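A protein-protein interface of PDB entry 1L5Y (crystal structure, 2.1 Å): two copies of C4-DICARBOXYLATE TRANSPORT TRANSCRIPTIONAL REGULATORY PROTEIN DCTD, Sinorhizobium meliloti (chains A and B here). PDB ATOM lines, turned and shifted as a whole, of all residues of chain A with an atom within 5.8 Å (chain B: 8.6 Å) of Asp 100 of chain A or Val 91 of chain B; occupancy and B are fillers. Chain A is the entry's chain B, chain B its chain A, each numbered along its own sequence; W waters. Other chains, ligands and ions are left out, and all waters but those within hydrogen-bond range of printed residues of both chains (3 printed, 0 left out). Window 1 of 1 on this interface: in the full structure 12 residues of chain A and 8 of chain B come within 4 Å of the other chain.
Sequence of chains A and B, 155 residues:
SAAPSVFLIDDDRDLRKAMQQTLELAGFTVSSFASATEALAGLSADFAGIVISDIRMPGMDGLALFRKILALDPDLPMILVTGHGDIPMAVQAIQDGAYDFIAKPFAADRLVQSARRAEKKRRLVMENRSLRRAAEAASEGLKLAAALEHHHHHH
Hydrophobic or aromatic side chains of chain A within 4 Å of the printed part of chain B: Ala 90, Val 91, Ile 94 and Phe 101. Of the 14 printed residues of chain B, 6 touch a printed residue of chain A. Hydrophobic or aromatic side chains of chain B within 4 Å of the printed part of chain A: Ile 87, Pro 88, Val 91 and Ile 94. Among the printed residues, 11 pairs touch across the chains. Among the printed residues, no Asp or Glu carboxylate lies within 4 Å of a Lys or Arg side-chain nitrogen of the other chain.
Asp 100 of chain A touches just one residue of chain B: Val 91. Printed residues of chain A within 4 Å of Val 91 of chain B: Ile 94 (3.99 Å), Asp 100 (3.8 Å) and Phe 101 (3.7 Å). Of the printed residues of chain B, Ala 90 of chain A touches Ile 87 (3.9 Å). Of the printed residues of chain B, Phe 101 of chain A touches Ile 87 and Val 91. Of the printed residues of chain A, Ile 87 of chain B touches Ala 90 (3.9 Å) and Phe 101 (3.7 Å). Of the printed residues of chain B, Arg 110 of chain A touches Pro 88 (3.6 Å). Of the printed residues of chain B, Val 91 of chain A touches Ile 94 (3.9 Å) and Phe 101 (3.8 Å). The nearest residue of chain B that does not touch Asp 100 of chain A is Gln 95 of chain B (4.6 Å). The nearest printed residue of chain A that does not touch Val 91 of chain B is Ala 90 of chain A (4.2 Å). The nearest printed residue of chain A that does not touch Phe 101 of chain B is Ala 90 of chain A (7.9 Å).
Water W1 lies within hydrogen-bond range of the backbone carbonyl oxygen (O) of Pro 88 of chain B (2.8 Å), the side-chain amide oxygen (OE1) of Gln 92 of chain B (3.0 Å) and the guanidinium group (NH1) of Arg 110 of chain A (3.4 Å). Water W3 lies within hydrogen-bond range of NE2 of Gln 95 of chain B (2.8 Å) and O of Ala 98 of chain A (3.4 Å). Water W2 bridges O of Tyr 99 of chain A (3.0 Å) and NE2 of Gln 95 of chain B (3.0 Å).
Among the printed residues, pairs that only touch across the chains: Arg 110 of chain A with Pro 88 of chain B (3.6 Å), Ile 94 of chain A with Ile 94 of chain B (3.6 Å), Phe 101 of chain A with Val 91 of chain B (3.7 Å), Phe 101 of chain A with Ile 87 of chain B (3.7 Å), Val 91 of chain A with Phe 101 of chain B (3.8 Å), Asp 100 of chain A with Val 91 of chain B (3.8 Å), Ala 90 of chain A with Ile 87 of chain B (3.9 Å), Val 91 of chain A with Ile 94 of chain B (3.9 Å), Ile 94 of chain A with Gln 95 of chain B (3.9 Å) and Ile 94 of chain A with Val 91 of chain B (3.99 Å).
The backbone carbonyl oxygen of Met 78 of chain A is in hydrogen-bond range of the backbone NH of Tyr 99 of chain A. The backbone NH (N) of Leu 80 of chain A sits at hydrogen-bond distance from the backbone carbonyl oxygen (O) of Asp 100 of chain A, 3.0 Å away. The side-chain hydroxyl (OG) of Ser 114 of chain A is in hydrogen-bond range of the side-chain carboxylate (OD2) of Asp 100 of chain A, at 2.7 Å.
Val 91 of chain A touches Ile 94 of chain B, and with the chains exchanged Ile 94 of chain A touches Val 91 of chain B. Val 91 of chain A touches Phe 101 of chain B, and with the chains exchanged Phe 101 of chain A touches Val 91 of chain B. Ile 94 of chain B touches its own counterpart, Ile 94 of chain A. Of the 11 pairs that touch across the chains among the printed residues, 5 have their exchanged pair printed and touching as well.
The backbone carbonyl oxygen (O) of Tyr 99 of chain A is in hydrogen-bond range of the side-chain amide nitrogen (NE2) of Gln 95 of chain B, 3.3 Å away.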
ATOM      1  N   MET A  78     -39.358  11.252   1.363  1.00  0.00           N
ATOM      2  CA  MET A  78     -39.050  10.540   0.130  1.00  0.00           C
ATOM      3  C   MET A  78     -37.779   9.710   0.293  1.00  0.00           C
ATOM      4  O   MET A  78     -36.748  10.187   0.797  1.00  0.00           O
ATOM      5  CB  MET A  78     -38.884  11.467  -1.058  1.00  0.00           C
ATOM      6  CG  MET A  78     -38.713  10.657  -2.367  1.00  0.00           C
ATOM      7  SD  MET A  78     -38.765  11.736  -3.773  1.00  0.00           S
ATOM      8  CE  MET A  78     -38.559  10.620  -5.188  1.00  0.00           C
ATOM      9  N   ILE A  79     -37.889   8.449  -0.116  1.00  0.00           N
ATOM     10  CA  ILE A  79     -36.800   7.494  -0.062  1.00  0.00           C
ATOM     11  C   ILE A  79     -36.429   7.154  -1.499  1.00  0.00           C
ATOM     12  O   ILE A  79     -37.302   6.781  -2.289  1.00  0.00           O
ATOM     13  CB  ILE A  79     -37.242   6.200   0.638  1.00  0.00           C
ATOM     14  CG1 ILE A  79     -37.440   6.499   2.131  1.00  0.00           C
ATOM     15  CG2 ILE A  79     -36.224   5.067   0.368  1.00  0.00           C
ATOM     16  CD1 ILE A  79     -37.971   5.326   2.952  1.00  0.00           C
ATOM     17  N   LEU A  80     -35.149   7.298  -1.835  1.00  0.00           N
ATOM     18  CA  LEU A  80     -34.676   6.976  -3.179  1.00  0.00           C
ATOM     19  C   LEU A  80     -33.984   5.634  -3.158  1.00  0.00           C
ATOM     20  O   LEU A  80     -33.256   5.302  -2.217  1.00  0.00           O
ATOM     21  CB  LEU A  80     -33.702   8.041  -3.700  1.00  0.00           C
ATOM     22  CG  LEU A  80     -34.317   9.433  -3.885  1.00  0.00           C
ATOM     23  CD1 LEU A  80     -33.210  10.463  -3.764  1.00  0.00           C
ATOM     24  CD2 LEU A  80     -35.043   9.541  -5.222  1.00  0.00           C
ATOM     25  N   VAL A  81     -34.201   4.870  -4.222  1.00  0.00           N
ATOM     26  CA  VAL A  81     -33.616   3.539  -4.354  1.00  0.00           C
ATOM     27  C   VAL A  81     -33.072   3.459  -5.762  1.00  0.00           C
ATOM     28  O   VAL A  81     -33.781   3.749  -6.713  1.00  0.00           O
ATOM     29  CB  VAL A  81     -34.698   2.438  -4.154  1.00  0.00           C
ATOM     30  CG1 VAL A  81     -34.043   1.080  -4.142  1.00  0.00           C
ATOM     31  CG2 VAL A  81     -35.472   2.675  -2.835  1.00  0.00           C
ATOM     32  N   ALA A  90     -25.571  10.007  -3.468  1.00  0.00           N
ATOM     33  CA  ALA A  90     -26.191   9.644  -2.205  1.00  0.00           C
ATOM     34  C   ALA A  90     -25.977  10.751  -1.160  1.00  0.00           C
ATOM     35  O   ALA A  90     -26.914  11.148  -0.466  1.00  0.00           O
ATOM     36  CB  ALA A  90     -25.619   8.325  -1.718  1.00  0.00           C
ATOM     37  N   VAL A  91     -24.742  11.236  -1.033  1.00  0.00           N
ATOM     38  CA  VAL A  91     -24.441  12.318  -0.080  1.00  0.00           C
ATOM     39  C   VAL A  91     -25.244  13.587  -0.415  1.00  0.00           C
ATOM     40  O   VAL A  91     -25.858  14.227   0.451  1.00  0.00           O
ATOM     41  CB  VAL A  91     -22.929  12.670  -0.109  1.00  0.00           C
ATOM     42  CG1 VAL A  91     -22.648  13.964   0.724  1.00  0.00           C
ATOM     43  CG2 VAL A  91     -22.137  11.496   0.429  1.00  0.00           C
ATOM     44  N   ILE A  94     -29.027  13.106   0.389  1.00  0.00           N
ATOM     45  CA  ILE A  94     -29.309  13.215   1.825  1.00  0.00           C
ATOM     46  C   ILE A  94     -29.234  14.673   2.317  1.00  0.00           C
ATOM     47  O   ILE A  94     -30.072  15.139   3.084  1.00  0.00           O
ATOM     48  CB  ILE A  94     -28.298  12.378   2.638  1.00  0.00           C
ATOM     49  CG1 ILE A  94     -28.478  10.907   2.286  1.00  0.00           C
ATOM     50  CG2 ILE A  94     -28.551  12.564   4.158  1.00  0.00           C
ATOM     51  CD1 ILE A  94     -29.865  10.390   2.579  1.00  0.00           C
ATOM     52  N   ALA A  98     -33.328  14.120   1.303  1.00  0.00           N
ATOM     53  CA  ALA A  98     -33.978  12.842   1.025  1.00  0.00           C
ATOM     54  C   ALA A  98     -34.015  12.067   2.339  1.00  0.00           C
ATOM     55  O   ALA A  98     -33.090  12.159   3.168  1.00  0.00           O
ATOM     56  CB  ALA A  98     -33.199  12.054  -0.011  1.00  0.00           C
ATOM     57  N   TYR A  99     -35.087  11.314   2.544  1.00  0.00           N
ATOM     58  CA  TYR A  99     -35.190  10.558   3.764  1.00  0.00           C
ATOM     59  C   TYR A  99     -34.204   9.382   3.841  1.00  0.00           C
ATOM     60  O   TYR A  99     -33.697   9.061   4.911  1.00  0.00           O
ATOM     61  CB  TYR A  99     -36.617  10.085   3.951  1.00  0.00           C
ATOM     62  CG  TYR A  99     -36.807   9.471   5.288  1.00  0.00           C
ATOM     63  CD1 TYR A  99     -36.530   8.132   5.485  1.00  0.00           C
ATOM     64  CD2 TYR A  99     -37.163  10.248   6.397  1.00  0.00           C
ATOM     65  CE1 TYR A  99     -36.584   7.562   6.736  1.00  0.00           C
ATOM     66  CE2 TYR A  99     -37.223   9.674   7.672  1.00  0.00           C
ATOM     67  CZ  TYR A  99     -36.928   8.328   7.817  1.00  0.00           C
ATOM     68  OH  TYR A  99     -36.972   7.713   9.039  1.00  0.00           O
ATOM     69  N   ASP A 100     -33.954   8.713   2.725  1.00  0.00           N
ATOM     70  CA  ASP A 100     -32.980   7.619   2.730  1.00  0.00           C
ATOM     71  C   ASP A 100     -32.572   7.474   1.263  1.00  0.00           C
ATOM     72  O   ASP A 100     -33.268   7.976   0.376  1.00  0.00           O
ATOM     73  CB  ASP A 100     -33.594   6.305   3.254  1.00  0.00           C
ATOM     74  CG  ASP A 100     -32.550   5.355   3.804  1.00  0.00           C
ATOM     75  OD1 ASP A 100     -31.335   5.578   3.600  1.00  0.00           O
ATOM     76  OD2 ASP A 100     -32.916   4.377   4.453  1.00  0.00           O
ATOM     77  N   PHE A 101     -31.433   6.851   1.008  1.00  0.00           N
ATOM     78  CA  PHE A 101     -30.955   6.669  -0.364  1.00  0.00           C
ATOM     79  C   PHE A 101     -30.375   5.264  -0.304  1.00  0.00           C
ATOM     80  O   PHE A 101     -29.364   5.005   0.361  1.00  0.00           O
ATOM     81  CB  PHE A 101     -29.882   7.720  -0.692  1.00  0.00           C
ATOM     82  CG  PHE A 101     -29.394   7.675  -2.123  1.00  0.00           C
ATOM     83  CD1 PHE A 101     -28.493   6.685  -2.536  1.00  0.00           C
ATOM     84  CD2 PHE A 101     -29.827   8.643  -3.056  1.00  0.00           C
ATOM     85  CE1 PHE A 101     -28.028   6.658  -3.849  1.00  0.00           C
ATOM     86  CE2 PHE A 101     -29.370   8.635  -4.392  1.00  0.00           C
ATOM     87  CZ  PHE A 101     -28.470   7.647  -4.791  1.00  0.00           C
ATOM     88  N   ILE A 102     -31.037   4.353  -0.987  1.00  0.00           N
ATOM     89  CA  ILE A 102     -30.678   2.952  -0.928  1.00  0.00           C
ATOM     90  C   ILE A 102     -30.209   2.411  -2.250  1.00  0.00           C
ATOM     91  O   ILE A 102     -30.761   2.732  -3.304  1.00  0.00           O
ATOM     92  CB  ILE A 102     -31.923   2.167  -0.402  1.00  0.00           C
ATOM     93  CG1 ILE A 102     -32.264   2.682   1.007  1.00  0.00           C
ATOM     94  CG2 ILE A 102     -31.709   0.664  -0.489  1.00  0.00           C
ATOM     95  CD1 ILE A 102     -33.638   2.187   1.561  1.00  0.00           C
ATOM     96  N   ARG A 110     -33.768  -3.152   5.463  1.00  0.00           N
ATOM     97  CA  ARG A 110     -33.306  -1.769   5.476  1.00  0.00           C
ATOM     98  C   ARG A 110     -34.441  -0.913   4.908  1.00  0.00           C
ATOM     99  O   ARG A 110     -34.799   0.130   5.475  1.00  0.00           O
ATOM    100  CB  ARG A 110     -32.074  -1.575   4.581  1.00  0.00           C
ATOM    101  CG  ARG A 110     -31.648  -0.112   4.428  1.00  0.00           C
ATOM    102  CD  ARG A 110     -30.506   0.081   3.414  1.00  0.00           C
ATOM    103  NE  ARG A 110     -29.310  -0.654   3.814  1.00  0.00           N
ATOM    104  CZ  ARG A 110     -28.395  -0.210   4.677  1.00  0.00           C
ATOM    105  NH1 ARG A 110     -28.505   1.001   5.241  1.00  0.00           N
ATOM    106  NH2 ARG A 110     -27.383  -1.009   5.015  1.00  0.00           N
ATOM    107  N   SER A 114     -36.836   1.633   7.287  1.00  0.00           N
ATOM    108  CA  SER A 114     -36.718   3.015   6.894  1.00  0.00           C
ATOM    109  C   SER A 114     -38.100   3.577   6.483  1.00  0.00           C
ATOM    110  O   SER A 114     -38.468   4.689   6.876  1.00  0.00           O
ATOM    111  CB  SER A 114     -35.725   3.099   5.750  1.00  0.00           C
ATOM    112  OG  SER A 114     -35.322   4.428   5.629  1.00  0.00           O
ATOM    113  N   ASP B  86     -18.994   2.922   0.693  1.00  0.00           N
ATOM    114  CA  ASP B  86     -20.116   2.470  -0.133  1.00  0.00           C
ATOM    115  C   ASP B  86     -21.263   3.411   0.208  1.00  0.00           C
ATOM    116  O   ASP B  86     -21.111   4.298   1.070  1.00  0.00           O
ATOM    117  CB  ASP B  86     -20.494   1.006   0.122  1.00  0.00           C
ATOM    118  CG  ASP B  86     -20.887   0.729   1.556  1.00  0.00           C
ATOM    119  OD1 ASP B  86     -21.232   1.655   2.318  1.00  0.00           O
ATOM    120  OD2 ASP B  86     -20.871  -0.462   1.916  1.00  0.00           O
ATOM    121  N   ILE B  87     -22.397   3.246  -0.462  1.00  0.00           N
ATOM    122  CA  ILE B  87     -23.541   4.131  -0.244  1.00  0.00           C
ATOM    123  C   ILE B  87     -24.131   4.123   1.176  1.00  0.00           C
ATOM    124  O   ILE B  87     -24.349   5.198   1.756  1.00  0.00           O
ATOM    125  CB  ILE B  87     -24.611   3.869  -1.338  1.00  0.00           C
ATOM    126  CG1 ILE B  87     -24.081   4.425  -2.687  1.00  0.00           C
ATOM    127  CG2 ILE B  87     -25.934   4.547  -0.970  1.00  0.00           C
ATOM    128  CD1 ILE B  87     -24.692   3.842  -3.947  1.00  0.00           C
ATOM    129  N   PRO B  88     -24.384   2.931   1.767  1.00  0.00           N
ATOM    130  CA  PRO B  88     -24.943   2.910   3.121  1.00  0.00           C
ATOM    131  C   PRO B  88     -24.047   3.547   4.185  1.00  0.00           C
ATOM    132  O   PRO B  88     -24.534   4.187   5.125  1.00  0.00           O
ATOM    133  CB  PRO B  88     -25.220   1.410   3.383  1.00  0.00           C
ATOM    134  CG  PRO B  88     -24.427   0.671   2.321  1.00  0.00           C
ATOM    135  CD  PRO B  88     -24.519   1.608   1.134  1.00  0.00           C
ATOM    136  N   MET B  89     -22.741   3.378   4.039  1.00  0.00           N
ATOM    137  CA  MET B  89     -21.814   3.963   4.981  1.00  0.00           C
ATOM    138  C   MET B  89     -21.819   5.509   4.860  1.00  0.00           C
ATOM    139  O   MET B  89     -21.851   6.198   5.859  1.00  0.00           O
ATOM    140  CB  MET B  89     -20.422   3.425   4.689  1.00  0.00           C
ATOM    141  CG  MET B  89     -19.329   3.890   5.600  1.00  0.00           C
ATOM    142  SD  MET B  89     -17.754   3.446   4.847  1.00  0.00           S
ATOM    143  CE  MET B  89     -17.800   1.694   4.844  1.00  0.00           C
ATOM    144  N   ALA B  90     -21.794   6.047   3.634  1.00  0.00           N
ATOM    145  CA  ALA B  90     -21.786   7.510   3.402  1.00  0.00           C
ATOM    146  C   ALA B  90     -23.071   8.169   3.877  1.00  0.00           C
ATOM    147  O   ALA B  90     -23.052   9.244   4.489  1.00  0.00           O
ATOM    148  CB  ALA B  90     -21.587   7.775   1.913  1.00  0.00           C
ATOM    149  N   VAL B  91     -24.197   7.525   3.572  1.00  0.00           N
ATOM    150  CA  VAL B  91     -25.517   7.991   3.990  1.00  0.00           C
ATOM    151  C   VAL B  91     -25.550   8.083   5.499  1.00  0.00           C
ATOM    152  O   VAL B  91     -25.956   9.098   6.051  1.00  0.00           O
ATOM    153  CB  VAL B  91     -26.670   7.003   3.535  1.00  0.00           C
ATOM    154  CG1 VAL B  91     -27.943   7.231   4.346  1.00  0.00           C
ATOM    155  CG2 VAL B  91     -26.982   7.217   2.048  1.00  0.00           C
ATOM    156  N   GLN B  92     -25.095   7.025   6.181  1.00  0.00           N
ATOM    157  CA  GLN B  92     -25.156   7.043   7.634  1.00  0.00           C
ATOM    158  C   GLN B  92     -24.249   8.095   8.246  1.00  0.00           C
ATOM    159  O   GLN B  92     -24.617   8.715   9.230  1.00  0.00           O
ATOM    160  CB  GLN B  92     -24.822   5.673   8.230  1.00  0.00           C
ATOM    161  CG  GLN B  92     -25.333   5.543   9.656  1.00  0.00           C
ATOM    162  CD  GLN B  92     -26.834   5.638   9.701  1.00  0.00           C
ATOM    163  OE1 GLN B  92     -27.532   5.126   8.800  1.00  0.00           O
ATOM    164  NE2 GLN B  92     -27.356   6.291  10.733  1.00  0.00           N
ATOM    165  N   ALA B  93     -23.066   8.280   7.674  1.00  0.00           N
ATOM    166  CA  ALA B  93     -22.137   9.278   8.178  1.00  0.00           C
ATOM    167  C   ALA B  93     -22.759  10.665   8.116  1.00  0.00           C
ATOM    168  O   ALA B  93     -22.679  11.415   9.083  1.00  0.00           O
ATOM    169  CB  ALA B  93     -20.852   9.261   7.374  1.00  0.00           C
ATOM    170  N   ILE B  94     -23.367  11.004   6.980  1.00  0.00           N
ATOM    171  CA  ILE B  94     -23.985  12.324   6.819  1.00  0.00           C
ATOM    172  C   ILE B  94     -25.180  12.437   7.784  1.00  0.00           C
ATOM    173  O   ILE B  94     -25.352  13.450   8.466  1.00  0.00           O
ATOM    174  CB  ILE B  94     -24.481  12.545   5.355  1.00  0.00           C
ATOM    175  CG1 ILE B  94     -23.293  12.547   4.384  1.00  0.00           C
ATOM    176  CG2 ILE B  94     -25.316  13.838   5.254  1.00  0.00           C
ATOM    177  CD1 ILE B  94     -22.273  13.666   4.590  1.00  0.00           C
ATOM    178  N   GLN B  95     -25.993  11.388   7.872  1.00  0.00           N
ATOM    179  CA  GLN B  95     -27.126  11.447   8.792  1.00  0.00           C
ATOM    180  C   GLN B  95     -26.652  11.572  10.237  1.00  0.00           C
ATOM    181  O   GLN B  95     -27.282  12.258  11.036  1.00  0.00           O
ATOM    182  CB  GLN B  95     -28.020  10.233   8.629  1.00  0.00           C
ATOM    183  CG  GLN B  95     -28.801  10.225   7.299  1.00  0.00           C
ATOM    184  CD  GLN B  95     -29.708   9.032   7.210  1.00  0.00           C
ATOM    185  OE1 GLN B  95     -29.375   7.969   7.714  1.00  0.00           O
ATOM    186  NE2 GLN B  95     -30.860   9.191   6.555  1.00  0.00           N
ATOM    187  N   ASP B  96     -25.528  10.955  10.569  1.00  0.00           N
ATOM    188  CA  ASP B  96     -25.016  11.066  11.931  1.00  0.00           C
ATOM    189  C   ASP B  96     -24.329  12.400  12.205  1.00  0.00           C
ATOM    190  O   ASP B  96     -23.873  12.635  13.325  1.00  0.00           O
ATOM    191  CB  ASP B  96     -24.034   9.942  12.260  1.00  0.00           C
ATOM    192  CG  ASP B  96     -24.694   8.588  12.345  1.00  0.00           C
ATOM    193  OD1 ASP B  96     -25.939   8.518  12.470  1.00  0.00           O
ATOM    194  OD2 ASP B  96     -23.949   7.582  12.295  1.00  0.00           O
ATOM    195  N   GLY B  97     -24.238  13.266  11.198  1.00  0.00           N
ATOM    196  CA  GLY B  97     -23.616  14.554  11.439  1.00  0.00           C
ATOM    197  C   GLY B  97     -22.245  14.846  10.835  1.00  0.00           C
ATOM    198  O   GLY B  97     -21.665  15.874  11.133  1.00  0.00           O
ATOM    199  N   ALA B  98     -21.689  13.958  10.024  1.00  0.00           N
ATOM    200  CA  ALA B  98     -20.396  14.266   9.404  1.00  0.00           C
ATOM    201  C   ALA B  98     -20.595  15.510   8.521  1.00  0.00           C
ATOM    202  O   ALA B  98     -21.613  15.635   7.814  1.00  0.00           O
ATOM    203  CB  ALA B  98     -19.936  13.100   8.538  1.00  0.00           C
ATOM    204  N   PHE B 101     -18.559  13.761   3.254  1.00  0.00           N
ATOM    205  CA  PHE B 101     -18.087  12.395   3.048  1.00  0.00           C
ATOM    206  C   PHE B 101     -17.652  12.380   1.581  1.00  0.00           C
ATOM    207  O   PHE B 101     -18.480  12.492   0.676  1.00  0.00           O
ATOM    208  CB  PHE B 101     -19.225  11.383   3.328  1.00  0.00           C
ATOM    209  CG  PHE B 101     -18.781   9.946   3.278  1.00  0.00           C
ATOM    210  CD1 PHE B 101     -18.598   9.309   2.067  1.00  0.00           C
ATOM    211  CD2 PHE B 101     -18.571   9.225   4.447  1.00  0.00           C
ATOM    212  CE1 PHE B 101     -18.208   7.962   2.007  1.00  0.00           C
ATOM    213  CE2 PHE B 101     -18.179   7.871   4.408  1.00  0.00           C
ATOM    214  CZ  PHE B 101     -17.997   7.239   3.189  1.00  0.00           C
HETATM  215  O   HOH W   1     -27.197   4.099   6.001  1.00  0.00           O
HETATM  216  O   HOH W   2     -32.950   7.153   7.036  1.00  0.00           O
HETATM  217  O   HOH W   3     -31.500  11.923   6.217  1.00  0.00           O
